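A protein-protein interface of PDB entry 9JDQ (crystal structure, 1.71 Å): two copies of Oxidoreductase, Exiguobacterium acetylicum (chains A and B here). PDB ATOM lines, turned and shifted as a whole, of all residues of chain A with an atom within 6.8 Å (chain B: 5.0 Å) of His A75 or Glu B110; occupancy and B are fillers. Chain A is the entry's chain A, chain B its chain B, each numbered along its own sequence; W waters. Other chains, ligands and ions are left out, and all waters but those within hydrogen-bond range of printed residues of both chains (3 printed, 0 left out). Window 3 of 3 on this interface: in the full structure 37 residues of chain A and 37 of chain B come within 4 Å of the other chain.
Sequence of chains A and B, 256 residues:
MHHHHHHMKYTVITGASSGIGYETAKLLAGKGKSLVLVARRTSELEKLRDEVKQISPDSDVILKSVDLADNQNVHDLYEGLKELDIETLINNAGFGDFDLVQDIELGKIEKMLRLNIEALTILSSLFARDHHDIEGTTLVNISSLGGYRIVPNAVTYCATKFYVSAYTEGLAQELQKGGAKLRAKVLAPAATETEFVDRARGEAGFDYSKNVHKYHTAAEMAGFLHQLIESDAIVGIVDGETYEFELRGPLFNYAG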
ATOM      1  N   ASP A  70     -14.934 -20.160  -1.794  1.00  0.00           N
ATOM      2  CA  ASP A  70     -15.148 -19.136  -2.814  1.00  0.00           C
ATOM      3  C   ASP A  70     -13.797 -18.778  -3.431  1.00  0.00           C
ATOM      4  O   ASP A  70     -12.877 -18.394  -2.692  1.00  0.00           O
ATOM      5  CB  ASP A  70     -15.850 -17.935  -2.201  1.00  0.00           C
ATOM      6  CG  ASP A  70     -15.998 -16.759  -3.144  1.00  0.00           C
ATOM      7  OD1 ASP A  70     -15.016 -15.996  -3.298  1.00  0.00           O
ATOM      8  OD2 ASP A  70     -17.084 -16.636  -3.730  1.00  0.00           O
ATOM      9  N   ASN A  71     -13.679 -18.894  -4.767  1.00  0.00           N
ATOM     10  CA  ASN A  71     -12.371 -18.830  -5.405  1.00  0.00           C
ATOM     11  C   ASN A  71     -11.749 -17.439  -5.247  1.00  0.00           C
ATOM     12  O   ASN A  71     -10.547 -17.321  -5.036  1.00  0.00           O
ATOM     13  CB  ASN A  71     -12.380 -19.059  -6.905  1.00  0.00           C
ATOM     14  CG  ASN A  71     -12.722 -20.474  -7.294  1.00  0.00           C
ATOM     15  OD1 ASN A  71     -12.787 -21.387  -6.454  1.00  0.00           O
ATOM     16  ND2 ASN A  71     -12.919 -20.660  -8.577  1.00  0.00           N
ATOM     17  N   GLN A  72     -12.585 -16.395  -5.304  1.00  0.00           N
ATOM     18  CA  GLN A  72     -12.105 -15.035  -5.121  1.00  0.00           C
ATOM     19  C   GLN A  72     -11.491 -14.873  -3.727  1.00  0.00           C
ATOM     20  O   GLN A  72     -10.414 -14.270  -3.573  1.00  0.00           O
ATOM     21  CB  GLN A  72     -13.218 -14.025  -5.417  1.00  0.00           C
ATOM     22  CG  GLN A  72     -12.712 -12.584  -5.470  1.00  0.00           C
ATOM     23  CD  GLN A  72     -11.675 -12.400  -6.551  1.00  0.00           C
ATOM     24  OE1 GLN A  72     -11.933 -12.685  -7.731  1.00  0.00           O
ATOM     25  NE2 GLN A  72     -10.506 -11.897  -6.167  1.00  0.00           N
ATOM     26  N   ASN A  73     -12.149 -15.450  -2.710  1.00  0.00           N
ATOM     27  CA  ASN A  73     -11.675 -15.367  -1.335  1.00  0.00           C
ATOM     28  C   ASN A  73     -10.291 -16.002  -1.204  1.00  0.00           C
ATOM     29  O   ASN A  73      -9.467 -15.538  -0.413  1.00  0.00           O
ATOM     30  CB  ASN A  73     -12.569 -16.093  -0.333  1.00  0.00           C
ATOM     31  CG  ASN A  73     -13.846 -15.352  -0.027  1.00  0.00           C
ATOM     32  OD1 ASN A  73     -14.010 -14.195  -0.420  1.00  0.00           O
ATOM     33  ND2 ASN A  73     -14.755 -15.995   0.688  1.00  0.00           N
ATOM     34  N   VAL A  74     -10.024 -17.032  -2.012  1.00  0.00           N
ATOM     35  CA  VAL A  74      -8.751 -17.725  -1.948  1.00  0.00           C
ATOM     36  C   VAL A  74      -7.660 -16.843  -2.561  1.00  0.00           C
ATOM     37  O   VAL A  74      -6.577 -16.645  -1.998  1.00  0.00           O
ATOM     38  CB  VAL A  74      -8.827 -19.108  -2.621  1.00  0.00           C
ATOM     39  CG1 VAL A  74      -7.481 -19.813  -2.503  1.00  0.00           C
ATOM     40  CG2 VAL A  74      -9.955 -19.987  -2.088  1.00  0.00           C
ATOM     41  N   HIS A  75      -7.962 -16.263  -3.723  1.00  0.00           N
ATOM     42  CA  HIS A  75      -7.080 -15.284  -4.322  1.00  0.00           C
ATOM     43  C   HIS A  75      -6.782 -14.130  -3.349  1.00  0.00           C
ATOM     44  O   HIS A  75      -5.619 -13.745  -3.166  1.00  0.00           O
ATOM     45  CB  HIS A  75      -7.648 -14.800  -5.655  1.00  0.00           C
ATOM     46  CG  HIS A  75      -7.518 -15.702  -6.842  1.00  0.00           C
ATOM     47  ND1 HIS A  75      -6.472 -15.636  -7.739  1.00  0.00           N
ATOM     48  CD2 HIS A  75      -8.361 -16.644  -7.319  1.00  0.00           C
ATOM     49  CE1 HIS A  75      -6.701 -16.499  -8.739  1.00  0.00           C
ATOM     50  NE2 HIS A  75      -7.852 -17.115  -8.503  1.00  0.00           N
ATOM     51  N   ASP A  76      -7.826 -13.562  -2.733  1.00  0.00           N
ATOM     52  CA  ASP A  76      -7.633 -12.411  -1.859  1.00  0.00           C
ATOM     53  C   ASP A  76      -6.813 -12.815  -0.635  1.00  0.00           C
ATOM     54  O   ASP A  76      -5.968 -12.045  -0.154  1.00  0.00           O
ATOM     55  CB  ASP A  76      -8.968 -11.800  -1.471  1.00  0.00           C
ATOM     56  CG  ASP A  76      -9.817 -11.227  -2.588  1.00  0.00           C
ATOM     57  OD1 ASP A  76      -9.271 -11.010  -3.702  1.00  0.00           O
ATOM     58  OD2 ASP A  76     -11.027 -11.057  -2.325  1.00  0.00           O
ATOM     59  N   LEU A  77      -7.048 -14.030  -0.138  1.00  0.00           N
ATOM     60  CA  LEU A  77      -6.260 -14.525   0.980  1.00  0.00           C
ATOM     61  C   LEU A  77      -4.775 -14.457   0.605  1.00  0.00           C
ATOM     62  O   LEU A  77      -3.972 -13.840   1.310  1.00  0.00           O
ATOM     63  CB  LEU A  77      -6.682 -15.934   1.382  1.00  0.00           C
ATOM     64  CG  LEU A  77      -5.737 -16.665   2.338  1.00  0.00           C
ATOM     65  CD1 LEU A  77      -5.683 -16.005   3.723  1.00  0.00           C
ATOM     66  CD2 LEU A  77      -6.079 -18.154   2.448  1.00  0.00           C
ATOM     67  N   TYR A  78      -4.414 -15.070  -0.528  1.00  0.00           N
ATOM     68  CA  TYR A  78      -3.014 -15.206  -0.895  1.00  0.00           C
ATOM     69  C   TYR A  78      -2.372 -13.836  -1.101  1.00  0.00           C
ATOM     70  O   TYR A  78      -1.282 -13.591  -0.601  1.00  0.00           O
ATOM     71  CB  TYR A  78      -2.801 -16.101  -2.115  1.00  0.00           C
ATOM     72  CG  TYR A  78      -1.335 -16.486  -2.291  1.00  0.00           C
ATOM     73  CD1 TYR A  78      -0.799 -17.594  -1.646  1.00  0.00           C
ATOM     74  CD2 TYR A  78      -0.482 -15.738  -3.092  1.00  0.00           C
ATOM     75  CE1 TYR A  78       0.531 -17.963  -1.802  1.00  0.00           C
ATOM     76  CE2 TYR A  78       0.850 -16.081  -3.237  1.00  0.00           C
ATOM     77  CZ  TYR A  78       1.362 -17.200  -2.595  1.00  0.00           C
ATOM     78  OH  TYR A  78       2.685 -17.518  -2.694  1.00  0.00           O
ATOM     79  N   GLU A  79      -3.070 -12.934  -1.786  1.00  0.00           N
ATOM     80  CA  GLU A  79      -2.554 -11.596  -2.039  1.00  0.00           C
ATOM     81  C   GLU A  79      -2.242 -10.879  -0.730  1.00  0.00           C
ATOM     82  O   GLU A  79      -1.270 -10.130  -0.662  1.00  0.00           O
ATOM     83  CB  GLU A  79      -3.562 -10.818  -2.877  1.00  0.00           C
ATOM     84  CG  GLU A  79      -3.272  -9.320  -2.943  1.00  0.00           C
ATOM     85  CD  GLU A  79      -2.380  -8.822  -4.060  1.00  0.00           C
ATOM     86  OE1 GLU A  79      -1.209  -9.264  -4.193  1.00  0.00           O
ATOM     87  OE2 GLU A  79      -2.894  -7.933  -4.785  1.00  0.00           O
ATOM     88  N   GLY A  80      -3.062 -11.093   0.307  1.00  0.00           N
ATOM     89  CA  GLY A  80      -2.852 -10.441   1.591  1.00  0.00           C
ATOM     90  C   GLY A  80      -1.607 -10.915   2.341  1.00  0.00           C
ATOM     91  O   GLY A  80      -1.214 -10.284   3.325  1.00  0.00           O
ATOM     92  N   GLU A 118     -10.459 -26.977  -5.682  1.00  0.00           N
ATOM     93  CA  GLU A 118     -10.231 -25.662  -6.260  1.00  0.00           C
ATOM     94  C   GLU A 118      -9.377 -24.806  -5.320  1.00  0.00           C
ATOM     95  O   GLU A 118      -8.369 -24.202  -5.745  1.00  0.00           O
ATOM     96  CB  GLU A 118     -11.484 -24.867  -6.622  1.00  0.00           C
ATOM     97  CG  GLU A 118     -12.345 -25.411  -7.759  1.00  0.00           C
ATOM     98  CD  GLU A 118     -13.613 -24.592  -8.004  1.00  0.00           C
ATOM     99  OE1 GLU A 118     -13.963 -23.716  -7.217  1.00  0.00           O
ATOM    100  OE2 GLU A 118     -14.268 -24.754  -9.052  1.00  0.00           O
ATOM    101  N   THR A 121      -5.875 -26.147  -5.320  1.00  0.00           N
ATOM    102  CA  THR A 121      -5.179 -25.888  -6.573  1.00  0.00           C
ATOM    103  C   THR A 121      -4.726 -24.418  -6.676  1.00  0.00           C
ATOM    104  O   THR A 121      -3.617 -24.113  -7.174  1.00  0.00           O
ATOM    105  CB  THR A 121      -6.084 -26.323  -7.720  1.00  0.00           C
ATOM    106  OG1 THR A 121      -6.325 -27.729  -7.625  1.00  0.00           O
ATOM    107  CG2 THR A 121      -5.388 -26.198  -9.066  1.00  0.00           C
ATOM    108  N   ILE A 122      -5.645 -23.504  -6.342  1.00  0.00           N
ATOM    109  CA  ILE A 122      -5.367 -22.078  -6.380  1.00  0.00           C
ATOM    110  C   ILE A 122      -4.145 -21.756  -5.508  1.00  0.00           C
ATOM    111  O   ILE A 122      -3.188 -21.148  -5.984  1.00  0.00           O
ATOM    112  CB  ILE A 122      -6.629 -21.255  -6.006  1.00  0.00           C
ATOM    113  CG1 ILE A 122      -7.727 -21.424  -7.052  1.00  0.00           C
ATOM    114  CG2 ILE A 122      -6.280 -19.774  -5.827  1.00  0.00           C
ATOM    115  CD1 ILE A 122      -9.072 -20.861  -6.640  1.00  0.00           C
ATOM    116  N   LEU A 123      -4.137 -22.215  -4.239  1.00  0.00           N
ATOM    117  CA  LEU A 123      -3.055 -21.877  -3.328  1.00  0.00           C
ATOM    118  C   LEU A 123      -1.752 -22.584  -3.719  1.00  0.00           C
ATOM    119  O   LEU A 123      -0.685 -21.989  -3.638  1.00  0.00           O
ATOM    120  CB  LEU A 123      -3.444 -22.144  -1.872  1.00  0.00           C
ATOM    121  CG  LEU A 123      -4.510 -21.229  -1.269  1.00  0.00           C
ATOM    122  CD1 LEU A 123      -5.064 -21.788   0.054  1.00  0.00           C
ATOM    123  CD2 LEU A 123      -4.018 -19.819  -1.087  1.00  0.00           C
ATOM    124  N   LEU A 126      -0.470 -20.579  -6.759  1.00  0.00           N
ATOM    125  CA  LEU A 126       0.035 -19.282  -6.331  1.00  0.00           C
ATOM    126  C   LEU A 126       1.332 -19.426  -5.552  1.00  0.00           C
ATOM    127  O   LEU A 126       2.245 -18.596  -5.736  1.00  0.00           O
ATOM    128  CB  LEU A 126      -0.997 -18.469  -5.547  1.00  0.00           C
ATOM    129  CG  LEU A 126      -2.241 -18.072  -6.336  1.00  0.00           C
ATOM    130  CD1 LEU A 126      -3.238 -17.478  -5.385  1.00  0.00           C
ATOM    131  CD2 LEU A 126      -2.013 -17.097  -7.500  1.00  0.00           C
ATOM    132  N   ARG A 129       4.100 -20.306  -8.018  1.00  0.00           N
ATOM    133  CA  ARG A 129       4.404 -19.195  -8.901  1.00  0.00           C
ATOM    134  C   ARG A 129       5.512 -18.318  -8.312  1.00  0.00           C
ATOM    135  O   ARG A 129       6.355 -17.815  -9.063  1.00  0.00           O
ATOM    136  CB  ARG A 129       3.109 -18.398  -9.096  1.00  0.00           C
ATOM    137  CG  ARG A 129       3.190 -17.095  -9.872  1.00  0.00           C
ATOM    138  CD  ARG A 129       1.860 -16.337 -10.053  1.00  0.00           C
ATOM    139  NE  ARG A 129       0.871 -16.993 -10.921  1.00  0.00           N
ATOM    140  CZ  ARG A 129      -0.401 -16.589 -11.040  1.00  0.00           C
ATOM    141  NH1 ARG A 129      -0.842 -15.540 -10.367  1.00  0.00           N
ATOM    142  NH2 ARG A 129      -1.246 -17.268 -11.791  1.00  0.00           N
ATOM    143  N   LEU B 106      -4.661 -18.869 -13.914  1.00  0.00           N
ATOM    144  CA  LEU B 106      -5.628 -19.434 -12.981  1.00  0.00           C
ATOM    145  C   LEU B 106      -7.052 -19.323 -13.505  1.00  0.00           C
ATOM    146  O   LEU B 106      -7.892 -20.163 -13.154  1.00  0.00           O
ATOM    147  CB  LEU B 106      -5.479 -18.894 -11.552  1.00  0.00           C
ATOM    148  CG  LEU B 106      -4.504 -19.688 -10.680  1.00  0.00           C
ATOM    149  CD1 LEU B 106      -4.085 -18.914  -9.447  1.00  0.00           C
ATOM    150  CD2 LEU B 106      -5.124 -21.032 -10.275  1.00  0.00           C
ATOM    151  N   GLY B 107      -7.317 -18.355 -14.380  1.00  0.00           N
ATOM    152  CA  GLY B 107      -8.639 -18.202 -14.956  1.00  0.00           C
ATOM    153  C   GLY B 107      -9.016 -19.426 -15.777  1.00  0.00           C
ATOM    154  O   GLY B 107     -10.092 -20.002 -15.587  1.00  0.00           O
ATOM    155  N   LYS B 108      -8.089 -19.836 -16.645  1.00  0.00           N
ATOM    156  CA  LYS B 108      -8.263 -21.023 -17.454  1.00  0.00           C
ATOM    157  C   LYS B 108      -8.330 -22.289 -16.585  1.00  0.00           C
ATOM    158  O   LYS B 108      -9.125 -23.189 -16.882  1.00  0.00           O
ATOM    159  CB  LYS B 108      -7.129 -21.106 -18.482  1.00  0.00           C
ATOM    160  CG  LYS B 108      -7.349 -22.210 -19.513  1.00  0.00           C
ATOM    161  CD  LYS B 108      -6.123 -22.514 -20.364  1.00  0.00           C
ATOM    162  CE  LYS B 108      -6.287 -23.646 -21.308  1.00  0.00           C
ATOM    163  NZ  LYS B 108      -5.061 -23.823 -22.090  1.00  0.00           N
ATOM    164  N   ILE B 109      -7.468 -22.392 -15.557  1.00  0.00           N
ATOM    165  CA  ILE B 109      -7.375 -23.640 -14.797  1.00  0.00           C
ATOM    166  C   ILE B 109      -8.617 -23.763 -13.920  1.00  0.00           C
ATOM    167  O   ILE B 109      -9.268 -24.815 -13.844  1.00  0.00           O
ATOM    168  CB  ILE B 109      -6.022 -23.765 -14.043  1.00  0.00           C
ATOM    169  CG1 ILE B 109      -5.028 -24.576 -14.869  1.00  0.00           C
ATOM    170  CG2 ILE B 109      -6.161 -24.397 -12.647  1.00  0.00           C
ATOM    171  CD1 ILE B 109      -4.732 -24.053 -16.254  1.00  0.00           C
ATOM    172  N   GLU B 110      -9.032 -22.631 -13.349  1.00  0.00           N
ATOM    173  CA  GLU B 110     -10.274 -22.613 -12.625  1.00  0.00           C
ATOM    174  C   GLU B 110     -11.410 -23.105 -13.521  1.00  0.00           C
ATOM    175  O   GLU B 110     -12.233 -23.893 -13.075  1.00  0.00           O
ATOM    176  CB  GLU B 110     -10.539 -21.229 -12.042  1.00  0.00           C
ATOM    177  CG  GLU B 110      -9.661 -21.008 -10.811  1.00  0.00           C
ATOM    178  CD  GLU B 110      -9.457 -19.561 -10.416  1.00  0.00           C
ATOM    179  OE1 GLU B 110     -10.238 -18.699 -10.909  1.00  0.00           O
ATOM    180  OE2 GLU B 110      -8.452 -19.327  -9.699  1.00  0.00           O
ATOM    181  N   LYS B 111     -11.520 -22.554 -14.740  1.00  0.00           N
ATOM    182  CA  LYS B 111     -12.555 -22.992 -15.663  1.00  0.00           C
ATOM    183  C   LYS B 111     -12.462 -24.491 -15.960  1.00  0.00           C
ATOM    184  O   LYS B 111     -13.489 -25.173 -16.075  1.00  0.00           O
ATOM    185  CB  LYS B 111     -12.453 -22.212 -16.975  1.00  0.00           C
ATOM    186  CG  LYS B 111     -13.686 -22.265 -17.824  1.00  0.00           C
ATOM    187  CD  LYS B 111     -13.546 -21.323 -19.012  1.00  0.00           C
ATOM    188  CE  LYS B 111     -14.789 -21.041 -19.782  1.00  0.00           C
ATOM    189  NZ  LYS B 111     -14.495 -20.310 -21.040  1.00  0.00           N
ATOM    190  N   MET B 112     -11.243 -24.980 -16.161  1.00  0.00           N
ATOM    191  CA  MET B 112     -11.008 -26.386 -16.414  1.00  0.00           C
ATOM    192  C   MET B 112     -11.565 -27.261 -15.285  1.00  0.00           C
ATOM    193  O   MET B 112     -12.114 -28.333 -15.548  1.00  0.00           O
ATOM    194  CB  MET B 112      -9.527 -26.689 -16.599  1.00  0.00           C
ATOM    195  CG  MET B 112      -9.259 -28.124 -17.079  1.00  0.00           C
ATOM    196  SD  MET B 112      -7.495 -28.534 -16.935  1.00  0.00           S
ATOM    197  CE  MET B 112      -6.886 -27.363 -18.132  1.00  0.00           C
ATOM    198  N   LEU B 113     -11.411 -26.803 -14.036  1.00  0.00           N
ATOM    199  CA  LEU B 113     -11.948 -27.528 -12.900  1.00  0.00           C
ATOM    200  C   LEU B 113     -13.479 -27.506 -12.984  1.00  0.00           C
ATOM    201  O   LEU B 113     -14.147 -28.528 -12.776  1.00  0.00           O
ATOM    202  CB  LEU B 113     -11.427 -26.930 -11.592  1.00  0.00           C
ATOM    203  CG  LEU B 113      -9.913 -26.951 -11.355  1.00  0.00           C
ATOM    204  CD1 LEU B 113      -9.493 -26.253 -10.076  1.00  0.00           C
ATOM    205  CD2 LEU B 113      -9.339 -28.287 -11.370  1.00  0.00           C
ATOM    206  N   ARG B 114     -14.055 -26.323 -13.217  1.00  0.00           N
ATOM    207  CA  ARG B 114     -15.509 -26.239 -13.362  1.00  0.00           C
ATOM    208  C   ARG B 114     -16.050 -27.141 -14.480  1.00  0.00           C
ATOM    209  O   ARG B 114     -17.160 -27.656 -14.356  1.00  0.00           O
ATOM    210  CB  ARG B 114     -15.947 -24.780 -13.535  1.00  0.00           C
ATOM    211  CG  ARG B 114     -15.582 -23.925 -12.333  1.00  0.00           C
ATOM    212  CD  ARG B 114     -16.277 -22.581 -12.400  1.00  0.00           C
ATOM    213  NE  ARG B 114     -16.044 -21.890 -13.672  1.00  0.00           N
ATOM    214  CZ  ARG B 114     -15.107 -20.956 -13.843  1.00  0.00           C
ATOM    215  NH1 ARG B 114     -14.242 -20.690 -12.869  1.00  0.00           N
ATOM    216  NH2 ARG B 114     -15.041 -20.315 -14.997  1.00  0.00           N
HETATM  217  O   HOH W   1     -13.957 -18.515 -10.257  1.00  0.00           O
HETATM  218  O   HOH W   2     -13.752 -22.395 -10.417  1.00  0.00           O
HETATM  219  O   HOH W   3     -10.156 -16.240 -10.642  1.00  0.00           O
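The side-chain carboxylate (OE2) of Glu B110 is in hydrogen-bond range of a ring nitrogen (NE2) of His A75, 2.6 Å away.
The backbone carbonyl oxygen (O) of Leu A126 is in hydrogen-bond range of the side-chain hydroxyl (OH) of Tyr A78, 3.3 Å away. The side-chain carboxylate (OE1) of Glu A118 sits close to the side-chain amide oxygen (OD1) of Asn A71, 2.7 Å away.
Among the printed residues, merely in contact across the chains: Asn A71 with Glu B110 (3.97 Å), His A75 with Leu B106 (3.6 Å), Glu A118 with Leu B113 (3.8 Å), Glu A118 with Arg B114 (3.6 Å), Ile A122 with Glu B110 (3.5 Å) and Leu A126 with Leu B106 (3.4 Å).
Of chain B, only Leu B106 and Glu B110 come within 4 Å of His A75. Of the printed residues of chain A, Glu B110 touches Asn A71, His A75 and Ile A122. Printed residues of chain A within 4 Å of Arg B114: Glu A118. Printed residues of chain A within 4 Å of Leu B113: Glu A118. Printed residues of chain B within 4 Å of Glu A118: Leu B113 (3.8 Å) and Arg B114 (3.6 Å). Printed residues of chain B within 4 Å of Ile A122: Glu B110. Of the printed residues of chain B, Asn A71 touches Glu B110. Leu A123 touches none of the printed residues of chain B. Lys B108 touches none of the printed residues of chain A. The nearest printed residue of chain B that does not touch His A75 is Gly B107 (6.0 Å). The nearest residue of chain A that does not touch Glu B110 is Glu A118 (4.6 Å). The nearest printed residue of chain A that does not touch Arg B114 is Asn A71 (4.5 Å).
Of the 17 printed residues of chain A, 5 touch a printed residue of chain B. Hydrophobic or aromatic side chains of chain A that line the printed part of chain B: His A75, Ile A122 and Leu A126. Among the printed residues, 7 pairs touch across the chains. Among the printed residues, no Asp or Glu carboxylate lies within 4 Å of a Lys or Arg side-chain nitrogen of the other chain.
No position is printed for both chains. Of the 7 pairs that touch across the chains among the printed residues, none has its exchanged pair printed and touching as well.
Water W3 bridges the side-chain carboxylate (OE1) of Glu B110 and a ring nitrogen (NE2) of His A75. Water W2 lies within hydrogen-bond range of ND2 of Asn A71 (2.7 Å), OE2 of Glu A118 (2.8 Å), NH1 of Arg B114 (3.0 Å) and O of Glu B110 (3.4 Å). Water W1 lies within hydrogen-bond range of the side-chain amide nitrogen (ND2) of Asn A71 (2.9 Å) and the guanidinium group (NH1) of Arg B114 (3.4 Å).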
